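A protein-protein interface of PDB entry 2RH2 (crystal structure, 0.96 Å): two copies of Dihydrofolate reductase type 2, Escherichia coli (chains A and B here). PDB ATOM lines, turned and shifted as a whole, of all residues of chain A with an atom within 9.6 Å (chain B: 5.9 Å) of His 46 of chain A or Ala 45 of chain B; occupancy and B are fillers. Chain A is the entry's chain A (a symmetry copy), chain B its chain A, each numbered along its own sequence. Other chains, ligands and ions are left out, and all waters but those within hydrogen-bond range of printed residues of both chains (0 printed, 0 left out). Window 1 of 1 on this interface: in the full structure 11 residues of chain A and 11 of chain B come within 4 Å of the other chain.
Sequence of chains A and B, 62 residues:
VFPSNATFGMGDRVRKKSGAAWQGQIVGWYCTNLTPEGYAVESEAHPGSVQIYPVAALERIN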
ATOM      1  N   ALA A  20       8.415  -1.948  -5.875  1.00  0.00           N
ATOM      2  CA  ALA A  20       8.341  -3.391  -5.664  1.00  0.00           C
ATOM      3  C   ALA A  20       9.309  -3.782  -4.554  1.00  0.00           C
ATOM      4  O   ALA A  20      10.471  -3.378  -4.531  1.00  0.00           O
ATOM      5  CB  ALA A  20       8.685  -4.113  -6.949  1.00  0.00           C
ATOM      6  N   ALA A  21       8.854  -4.651  -3.646  1.00  0.00           N
ATOM      7  CA  ALA A  21       9.656  -5.033  -2.504  1.00  0.00           C
ATOM      8  C   ALA A  21      10.592  -6.175  -2.839  1.00  0.00           C
ATOM      9  O   ALA A  21      10.297  -7.051  -3.675  1.00  0.00           O
ATOM     10  CB  ALA A  21       8.762  -5.419  -1.340  1.00  0.00           C
ATOM     11  N   TRP A  22      11.695  -6.240  -2.116  1.00  0.00           N
ATOM     12  CA  TRP A  22      12.598  -7.364  -2.234  1.00  0.00           C
ATOM     13  C   TRP A  22      13.531  -7.268  -1.036  1.00  0.00           C
ATOM     14  O   TRP A  22      13.947  -6.180  -0.686  1.00  0.00           O
ATOM     15  CB  TRP A  22      13.408  -7.281  -3.542  1.00  0.00           C
ATOM     16  CG  TRP A  22      14.069  -8.541  -3.865  1.00  0.00           C
ATOM     17  CD1 TRP A  22      15.414  -8.815  -3.825  1.00  0.00           C
ATOM     18  CD2 TRP A  22      13.429  -9.752  -4.305  1.00  0.00           C
ATOM     19  NE1 TRP A  22      15.651 -10.102  -4.237  1.00  0.00           N
ATOM     20  CE2 TRP A  22      14.453 -10.701  -4.547  1.00  0.00           C
ATOM     21  CE3 TRP A  22      12.094 -10.111  -4.556  1.00  0.00           C
ATOM     22  CZ2 TRP A  22      14.173 -11.993  -5.005  1.00  0.00           C
ATOM     23  CZ3 TRP A  22      11.818 -11.387  -5.039  1.00  0.00           C
ATOM     24  CH2 TRP A  22      12.857 -12.316  -5.248  1.00  0.00           C
ATOM     25  N   GLN A  23      13.908  -8.375  -0.417  1.00  0.00           N
ATOM     26  CA  GLN A  23      14.765  -8.331   0.773  1.00  0.00           C
ATOM     27  C   GLN A  23      15.508  -9.633   0.882  1.00  0.00           C
ATOM     28  O   GLN A  23      14.884 -10.711   0.746  1.00  0.00           O
ATOM     29  CB  GLN A  23      13.890  -8.059   1.995  1.00  0.00           C
ATOM     30  CG  GLN A  23      14.695  -7.813   3.279  1.00  0.00           C
ATOM     31  CD  GLN A  23      13.827  -7.209   4.335  1.00  0.00           C
ATOM     32  OE1 GLN A  23      13.312  -6.086   4.150  1.00  0.00           O
ATOM     33  NE2 GLN A  23      13.642  -7.911   5.433  1.00  0.00           N
ATOM     34  N   GLY A  24      16.796  -9.557   1.165  1.00  0.00           N
ATOM     35  CA  GLY A  24      17.614 -10.742   1.337  1.00  0.00           C
ATOM     36  C   GLY A  24      19.065 -10.396   1.232  1.00  0.00           C
ATOM     37  O   GLY A  24      19.473  -9.264   1.464  1.00  0.00           O
ATOM     38  N   GLN A  25      19.861 -11.414   0.883  1.00  0.00           N
ATOM     39  CA  GLN A  25      21.323 -11.312   0.906  1.00  0.00           C
ATOM     40  C   GLN A  25      21.902 -10.973  -0.489  1.00  0.00           C
ATOM     41  O   GLN A  25      21.496 -11.524  -1.509  1.00  0.00           O
ATOM     42  CB  GLN A  25      21.945 -12.630   1.334  1.00  0.00           C
ATOM     43  CG  GLN A  25      21.574 -13.001   2.743  1.00  0.00           C
ATOM     44  CD  GLN A  25      22.524 -13.980   3.377  1.00  0.00           C
ATOM     45  OE1 GLN A  25      22.162 -15.127   3.595  1.00  0.00           O
ATOM     46  NE2 GLN A  25      23.747 -13.535   3.672  1.00  0.00           N
ATOM     47  N   VAL A  41      20.437 -10.135  -5.569  1.00  0.00           N
ATOM     48  CA  VAL A  41      19.940 -10.301  -4.197  1.00  0.00           C
ATOM     49  C   VAL A  41      19.065 -11.565  -4.162  1.00  0.00           C
ATOM     50  O   VAL A  41      18.071 -11.651  -4.892  1.00  0.00           O
ATOM     51  CB  VAL A  41      19.097  -9.082  -3.766  1.00  0.00           C
ATOM     52  CG1 VAL A  41      18.689  -9.254  -2.286  1.00  0.00           C
ATOM     53  CG2 VAL A  41      19.872  -7.783  -3.955  1.00  0.00           C
ATOM     54  N   GLU A  42      19.422 -12.506  -3.293  1.00  0.00           N
ATOM     55  CA  GLU A  42      18.602 -13.700  -3.110  1.00  0.00           C
ATOM     56  C   GLU A  42      17.554 -13.409  -2.038  1.00  0.00           C
ATOM     57  O   GLU A  42      17.901 -12.968  -0.934  1.00  0.00           O
ATOM     58  CB  GLU A  42      19.477 -14.897  -2.678  1.00  0.00           C
ATOM     59  CG  GLU A  42      18.648 -16.176  -2.561  1.00  0.00           C
ATOM     60  CD  GLU A  42      19.432 -17.391  -2.178  1.00  0.00           C
ATOM     61  OE1 GLU A  42      20.628 -17.260  -1.789  1.00  0.00           O
ATOM     62  OE2 GLU A  42      18.868 -18.522  -2.237  1.00  0.00           O
ATOM     63  N   SER A  43      16.289 -13.617  -2.359  1.00  0.00           N
ATOM     64  CA  SER A  43      15.245 -13.384  -1.380  1.00  0.00           C
ATOM     65  C   SER A  43      15.435 -14.254  -0.142  1.00  0.00           C
ATOM     66  O   SER A  43      15.672 -15.461  -0.241  1.00  0.00           O
ATOM     67  CB  SER A  43      13.896 -13.727  -1.977  1.00  0.00           C
ATOM     68  OG  SER A  43      12.896 -13.715  -0.974  1.00  0.00           O
ATOM     69  N   GLU A  44      15.253 -13.638   1.032  1.00  0.00           N
ATOM     70  CA  GLU A  44      15.257 -14.374   2.288  1.00  0.00           C
ATOM     71  C   GLU A  44      13.924 -15.089   2.529  1.00  0.00           C
ATOM     72  O   GLU A  44      13.853 -15.979   3.380  1.00  0.00           O
ATOM     73  CB  GLU A  44      15.642 -13.482   3.465  1.00  0.00           C
ATOM     74  CG  GLU A  44      14.637 -12.406   3.772  1.00  0.00           C
ATOM     75  CD  GLU A  44      15.127 -11.344   4.724  1.00  0.00           C
ATOM     76  OE1 GLU A  44      16.358 -11.061   4.785  1.00  0.00           O
ATOM     77  OE2 GLU A  44      14.272 -10.718   5.395  1.00  0.00           O
ATOM     78  N   ALA A  45      12.878 -14.681   1.837  1.00  0.00           N
ATOM     79  CA  ALA A  45      11.578 -15.305   1.942  1.00  0.00           C
ATOM     80  C   ALA A  45      11.391 -16.446   0.967  1.00  0.00           C
ATOM     81  O   ALA A  45      10.662 -17.392   1.240  1.00  0.00           O
ATOM     82  CB  ALA A  45      10.486 -14.271   1.706  1.00  0.00           C
ATOM     83  N   HIS A  46      12.054 -16.352  -0.188  1.00  0.00           N
ATOM     84  CA  HIS A  46      11.893 -17.282  -1.300  1.00  0.00           C
ATOM     85  C   HIS A  46      13.266 -17.815  -1.703  1.00  0.00           C
ATOM     86  O   HIS A  46      13.862 -17.356  -2.691  1.00  0.00           O
ATOM     87  CB  HIS A  46      11.235 -16.597  -2.500  1.00  0.00           C
ATOM     88  CG  HIS A  46       9.889 -15.994  -2.246  1.00  0.00           C
ATOM     89  ND1 HIS A  46       8.832 -16.626  -1.644  1.00  0.00           N
ATOM     90  CD2 HIS A  46       9.400 -14.795  -2.591  1.00  0.00           C
ATOM     91  CE1 HIS A  46       7.783 -15.795  -1.648  1.00  0.00           C
ATOM     92  NE2 HIS A  46       8.093 -14.679  -2.224  1.00  0.00           N
ATOM     93  N   PRO A  47      13.791 -18.814  -1.001  1.00  0.00           N
ATOM     94  CA  PRO A  47      15.124 -19.349  -1.235  1.00  0.00           C
ATOM     95  C   PRO A  47      15.297 -19.707  -2.691  1.00  0.00           C
ATOM     96  O   PRO A  47      14.430 -20.350  -3.307  1.00  0.00           O
ATOM     97  CB  PRO A  47      15.180 -20.612  -0.331  1.00  0.00           C
ATOM     98  CG  PRO A  47      14.200 -20.379   0.645  1.00  0.00           C
ATOM     99  CD  PRO A  47      13.126 -19.518   0.111  1.00  0.00           C
ATOM    100  N   GLY A  48      16.456 -19.353  -3.243  1.00  0.00           N
ATOM    101  CA  GLY A  48      16.768 -19.705  -4.616  1.00  0.00           C
ATOM    102  C   GLY A  48      16.351 -18.669  -5.623  1.00  0.00           C
ATOM    103  O   GLY A  48      16.863 -18.702  -6.762  1.00  0.00           O
ATOM    104  N   SER A  49      15.382 -17.796  -5.307  1.00  0.00           N
ATOM    105  CA  SER A  49      14.963 -16.753  -6.248  1.00  0.00           C
ATOM    106  C   SER A  49      15.846 -15.524  -6.032  1.00  0.00           C
ATOM    107  O   SER A  49      15.964 -15.014  -4.925  1.00  0.00           O
ATOM    108  CB  SER A  49      13.519 -16.398  -6.065  1.00  0.00           C
ATOM    109  OG  SER A  49      12.746 -17.412  -6.612  1.00  0.00           O
ATOM    110  N   VAL A  50      16.440 -15.073  -7.132  1.00  0.00           N
ATOM    111  CA  VAL A  50      17.398 -13.979  -7.178  1.00  0.00           C
ATOM    112  C   VAL A  50      16.857 -12.926  -8.124  1.00  0.00           C
ATOM    113  O   VAL A  50      16.386 -13.261  -9.210  1.00  0.00           O
ATOM    114  CB  VAL A  50      18.771 -14.477  -7.672  1.00  0.00           C
ATOM    115  CG1 VAL A  50      19.784 -13.349  -7.738  1.00  0.00           C
ATOM    116  CG2 VAL A  50      19.303 -15.588  -6.755  1.00  0.00           C
ATOM    117  N   GLN A  51      17.020 -11.636  -7.758  1.00  0.00           N
ATOM    118  CA  GLN A  51      16.694 -10.535  -8.660  1.00  0.00           C
ATOM    119  C   GLN A  51      17.802  -9.539  -8.575  1.00  0.00           C
ATOM    120  O   GLN A  51      18.515  -9.425  -7.562  1.00  0.00           O
ATOM    121  CB  GLN A  51      15.310  -9.991  -8.357  1.00  0.00           C
ATOM    122  CG  GLN A  51      14.335 -11.098  -8.677  1.00  0.00           C
ATOM    123  CD  GLN A  51      12.901 -10.739  -8.716  1.00  0.00           C
ATOM    124  OE1 GLN A  51      12.126 -11.560  -9.148  1.00  0.00           O
ATOM    125  NE2 GLN A  51      12.524  -9.632  -8.122  1.00  0.00           N
ATOM    126  N   ALA B  20      13.808 -22.749  -7.452  1.00  0.00           N
ATOM    127  CA  ALA B  20      13.665 -21.423  -6.857  1.00  0.00           C
ATOM    128  C   ALA B  20      12.250 -21.273  -6.309  1.00  0.00           C
ATOM    129  O   ALA B  20      11.260 -21.584  -6.970  1.00  0.00           O
ATOM    130  CB  ALA B  20      13.947 -20.363  -7.898  1.00  0.00           C
ATOM    131  N   ALA B  21      12.136 -20.712  -5.101  1.00  0.00           N
ATOM    132  CA  ALA B  21      10.851 -20.592  -4.448  1.00  0.00           C
ATOM    133  C   ALA B  21      10.122 -19.338  -4.882  1.00  0.00           C
ATOM    134  O   ALA B  21      10.727 -18.295  -5.196  1.00  0.00           O
ATOM    135  CB  ALA B  21      11.026 -20.595  -2.941  1.00  0.00           C
ATOM    136  N   TRP B  22       8.805 -19.389  -4.808  1.00  0.00           N
ATOM    137  CA  TRP B  22       7.999 -18.213  -5.051  1.00  0.00           C
ATOM    138  C   TRP B  22       6.607 -18.557  -4.543  1.00  0.00           C
ATOM    139  O   TRP B  22       6.152 -19.666  -4.747  1.00  0.00           O
ATOM    140  CB  TRP B  22       7.946 -17.886  -6.556  1.00  0.00           C
ATOM    141  CG  TRP B  22       7.441 -16.541  -6.813  1.00  0.00           C
ATOM    142  CD1 TRP B  22       6.235 -16.192  -7.369  1.00  0.00           C
ATOM    143  CD2 TRP B  22       8.126 -15.306  -6.540  1.00  0.00           C
ATOM    144  NE1 TRP B  22       6.139 -14.828  -7.485  1.00  0.00           N
ATOM    145  CE2 TRP B  22       7.289 -14.256  -6.992  1.00  0.00           C
ATOM    146  CE3 TRP B  22       9.382 -14.990  -5.996  1.00  0.00           C
ATOM    147  CZ2 TRP B  22       7.664 -12.912  -6.890  1.00  0.00           C
ATOM    148  CZ3 TRP B  22       9.768 -13.655  -5.920  1.00  0.00           C
ATOM    149  CH2 TRP B  22       8.903 -12.631  -6.358  1.00  0.00           C
ATOM    150  N   GLN B  23       5.896 -17.630  -3.921  1.00  0.00           N
ATOM    151  CA  GLN B  23       4.569 -17.928  -3.368  1.00  0.00           C
ATOM    152  C   GLN B  23       3.778 -16.652  -3.297  1.00  0.00           C
ATOM    153  O   GLN B  23       4.309 -15.625  -2.815  1.00  0.00           O
ATOM    154  CB  GLN B  23       4.747 -18.578  -1.997  1.00  0.00           C
ATOM    155  CG  GLN B  23       3.434 -19.099  -1.394  1.00  0.00           C
ATOM    156  CD  GLN B  23       3.711 -20.022  -0.253  1.00  0.00           C
ATOM    157  OE1 GLN B  23       4.330 -21.090  -0.452  1.00  0.00           O
ATOM    158  NE2 GLN B  23       3.280 -19.654   0.935  1.00  0.00           N
ATOM    159  N   GLY B  24       2.527 -16.709  -3.715  1.00  0.00           N
ATOM    160  CA  GLY B  24       1.647 -15.556  -3.660  1.00  0.00           C
ATOM    161  C   GLY B  24       0.466 -15.758  -4.554  1.00  0.00           C
ATOM    162  O   GLY B  24       0.078 -16.878  -4.864  1.00  0.00           O
ATOM    163  N   SER B  43       4.410 -11.904  -5.306  1.00  0.00           N
ATOM    164  CA  SER B  43       4.851 -12.463  -4.043  1.00  0.00           C
ATOM    165  C   SER B  43       4.014 -11.943  -2.879  1.00  0.00           C
ATOM    166  O   SER B  43       3.771 -10.740  -2.756  1.00  0.00           O
ATOM    167  CB  SER B  43       6.291 -12.071  -3.783  1.00  0.00           C
ATOM    168  OG  SER B  43       6.665 -12.422  -2.462  1.00  0.00           O
ATOM    169  N   GLU B  44       3.639 -12.861  -1.980  1.00  0.00           N
ATOM    170  CA  GLU B  44       2.964 -12.487  -0.745  1.00  0.00           C
ATOM    171  C   GLU B  44       3.951 -11.960   0.301  1.00  0.00           C
ATOM    172  O   GLU B  44       3.530 -11.336   1.278  1.00  0.00           O
ATOM    173  CB  GLU B  44       2.116 -13.631  -0.197  1.00  0.00           C
ATOM    174  CG  GLU B  44       2.913 -14.818   0.266  1.00  0.00           C
ATOM    175  CD  GLU B  44       2.096 -16.058   0.531  1.00  0.00           C
ATOM    176  OE1 GLU B  44       1.017 -16.257  -0.100  1.00  0.00           O
ATOM    177  OE2 GLU B  44       2.552 -16.900   1.341  1.00  0.00           O
ATOM    178  N   ALA B  45       5.228 -12.243   0.134  1.00  0.00           N
ATOM    179  CA  ALA B  45       6.260 -11.764   1.026  1.00  0.00           C
ATOM    180  C   ALA B  45       6.820 -10.421   0.614  1.00  0.00           C
ATOM    181  O   ALA B  45       7.250  -9.637   1.451  1.00  0.00           O
ATOM    182  CB  ALA B  45       7.397 -12.774   1.093  1.00  0.00           C
ATOM    183  N   HIS B  46       6.820 -10.156  -0.695  1.00  0.00           N
ATOM    184  CA  HIS B  46       7.440  -8.978  -1.289  1.00  0.00           C
ATOM    185  C   HIS B  46       6.410  -8.260  -2.157  1.00  0.00           C
ATOM    186  O   HIS B  46       6.411  -8.396  -3.391  1.00  0.00           O
ATOM    187  CB  HIS B  46       8.651  -9.364  -2.143  1.00  0.00           C
ATOM    188  CG  HIS B  46       9.737 -10.108  -1.430  1.00  0.00           C
ATOM    189  ND1 HIS B  46      10.312  -9.736  -0.243  1.00  0.00           N
ATOM    190  CD2 HIS B  46      10.417 -11.203  -1.794  1.00  0.00           C
ATOM    191  CE1 HIS B  46      11.284 -10.610   0.049  1.00  0.00           C
ATOM    192  NE2 HIS B  46      11.378 -11.507  -0.879  1.00  0.00           N
ATOM    193  N   PRO B  47       5.536  -7.449  -1.568  1.00  0.00           N
ATOM    194  CA  PRO B  47       4.457  -6.777  -2.275  1.00  0.00           C
ATOM    195  C   PRO B  47       4.998  -6.033  -3.472  1.00  0.00           C
ATOM    196  O   PRO B  47       6.007  -5.313  -3.385  1.00  0.00           O
ATOM    197  CB  PRO B  47       3.873  -5.799  -1.218  1.00  0.00           C
ATOM    198  CG  PRO B  47       4.260  -6.354   0.012  1.00  0.00           C
ATOM    199  CD  PRO B  47       5.516  -7.116  -0.131  1.00  0.00           C
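NE2 of His 46 of chain B is in hydrogen-bond range of OG of Ser 43 of chain A (2.7 Å). The side-chain hydroxyl (OG) of Ser 49 of chain A lies within hydrogen-bond range of the backbone carbonyl oxygen (O) of Ala 21 of chain B (2.6 Å). O of Pro 47 of chain A lies within hydrogen-bond range of N of Ala 21 of chain B (2.9 Å). O of Pro 47 of chain B is in hydrogen-bond range of N of Ala 21 of chain A. NE2 of His 46 of chain A is in hydrogen-bond range of OG of Ser 43 of chain B (2.7 Å).
The side-chain carboxylate (OE2) of Glu 42 of chain A sits at hydrogen-bond distance from the backbone NH (N) of Gly 48 of chain A, 2.7 Å away. OG of Ser 43 of chain B lies within hydrogen-bond range of N of His 46 of chain B. The side-chain hydroxyl (OG) of Ser 43 of chain A is in hydrogen-bond range of the backbone NH (N) of Ala 45 of chain A (3.0 Å). N of Ser 43 of chain A lies within hydrogen-bond range of O of Ser 49 of chain A, at 2.9 Å. The side-chain hydroxyl of Ser 43 of chain A sits at hydrogen-bond distance from the backbone NH of His 46 of chain A (2.9 Å). OE2 of Glu 44 of chain B is in hydrogen-bond range of NE2 of Gln 23 of chain B (2.9 Å).
Ala 20 of chain A touches Pro 47 of chain B. Trp 22 of chain A touches Trp 22 of chain B. N of Gln 23 of chain A touches CE1 of His 46 of chain B, 3.5 Å away. Ala 45 of chain A touches Ala 45 of chain B. NE2 of His 46 of chain B touches CB of Ala 45 of chain A (3.9 Å). His 46 of chain A touches Ala 21 of chain B. Ala 45 of chain B touches His 46 of chain A (CB to NE2, 3.9 Å). Pro 47 of chain A touches Ala 20 of chain B. CB of Ala 20 of chain B touches O of Gly 48 of chain A, 3.5 Å away. Ser 49 of chain A touches Ala 20 of chain B (OG to CB, 3.4 Å).
Printed residues of chain B within 4 Å of His 46 of chain A: Ala 21 (3.2 Å), Trp 22 (3.4 Å), Gln 23 (3.5 Å), Ser 43 (2.7 Å), Ala 45 (3.9 Å) and His 46 (3.8 Å). Of the printed residues of chain A, Ala 45 of chain B touches Ala 45 and His 46. Ser 43 of chain B touches one residue of chain A. Of the printed residues of chain B, Ala 45 of chain A touches Ala 45 and His 46. Printed residues of chain A within 4 Å of Gln 23 of chain B: His 46 (3.5 Å). Printed residues of chain B within 4 Å of Trp 22 of chain A: Trp 22 and His 46. Printed residues of chain A within 4 Å of Ala 20 of chain B: Pro 47, Gly 48 and Ser 49. Of the printed residues of chain B, Pro 47 of chain A touches Ala 20 and Ala 21. The nearest printed residue of chain B that does not touch His 46 of chain A is Glu 44 of chain B (4.8 Å). The nearest residue of chain A that does not touch Ala 45 of chain B is Ala 21 of chain A (5.3 Å). The nearest printed residue of chain B that does not touch Trp 22 of chain A is Ser 43 of chain B (5.7 Å).
Of the 17 printed residues of chain A, 10 touch a printed residue of chain B. Hydrophobic or aromatic side chains of chain A that line the printed part of chain B: Ala 21, Trp 22, Ala 45, His 46 and Pro 47. Along chain A the printed residues that touch a printed residue of chain B span positions 20 to 49. Of the 10 printed residues of chain B, 8 touch a printed residue of chain A. Hydrophobic or aromatic side chains of chain B that line the printed part of chain A: Ala 20, Ala 21, Trp 22, Ala 45, His 46 and Pro 47. Among the printed residues, no Asp or Glu carboxylate lies within 4 Å of a Lys or Arg side-chain nitrogen of the other chain.
Ala 21 of chain A touches His 46 of chain B, and with the chains exchanged His 46 of chain A touches Ala 21 of chain B. Ala 21 of chain A touches Pro 47 of chain B, and with the chains exchanged Pro 47 of chain A touches Ala 21 of chain B. Trp 22 of chain A touches His 46 of chain B, and with the chains exchanged His 46 of chain A touches Trp 22 of chain B. Ser 43 of chain A touches His 46 of chain B, and with the chains exchanged His 46 of chain A touches Ser 43 of chain B. Of the 20 pairs that touch across the chains among the printed residues, 17 have their exchanged pair printed and touching as well.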
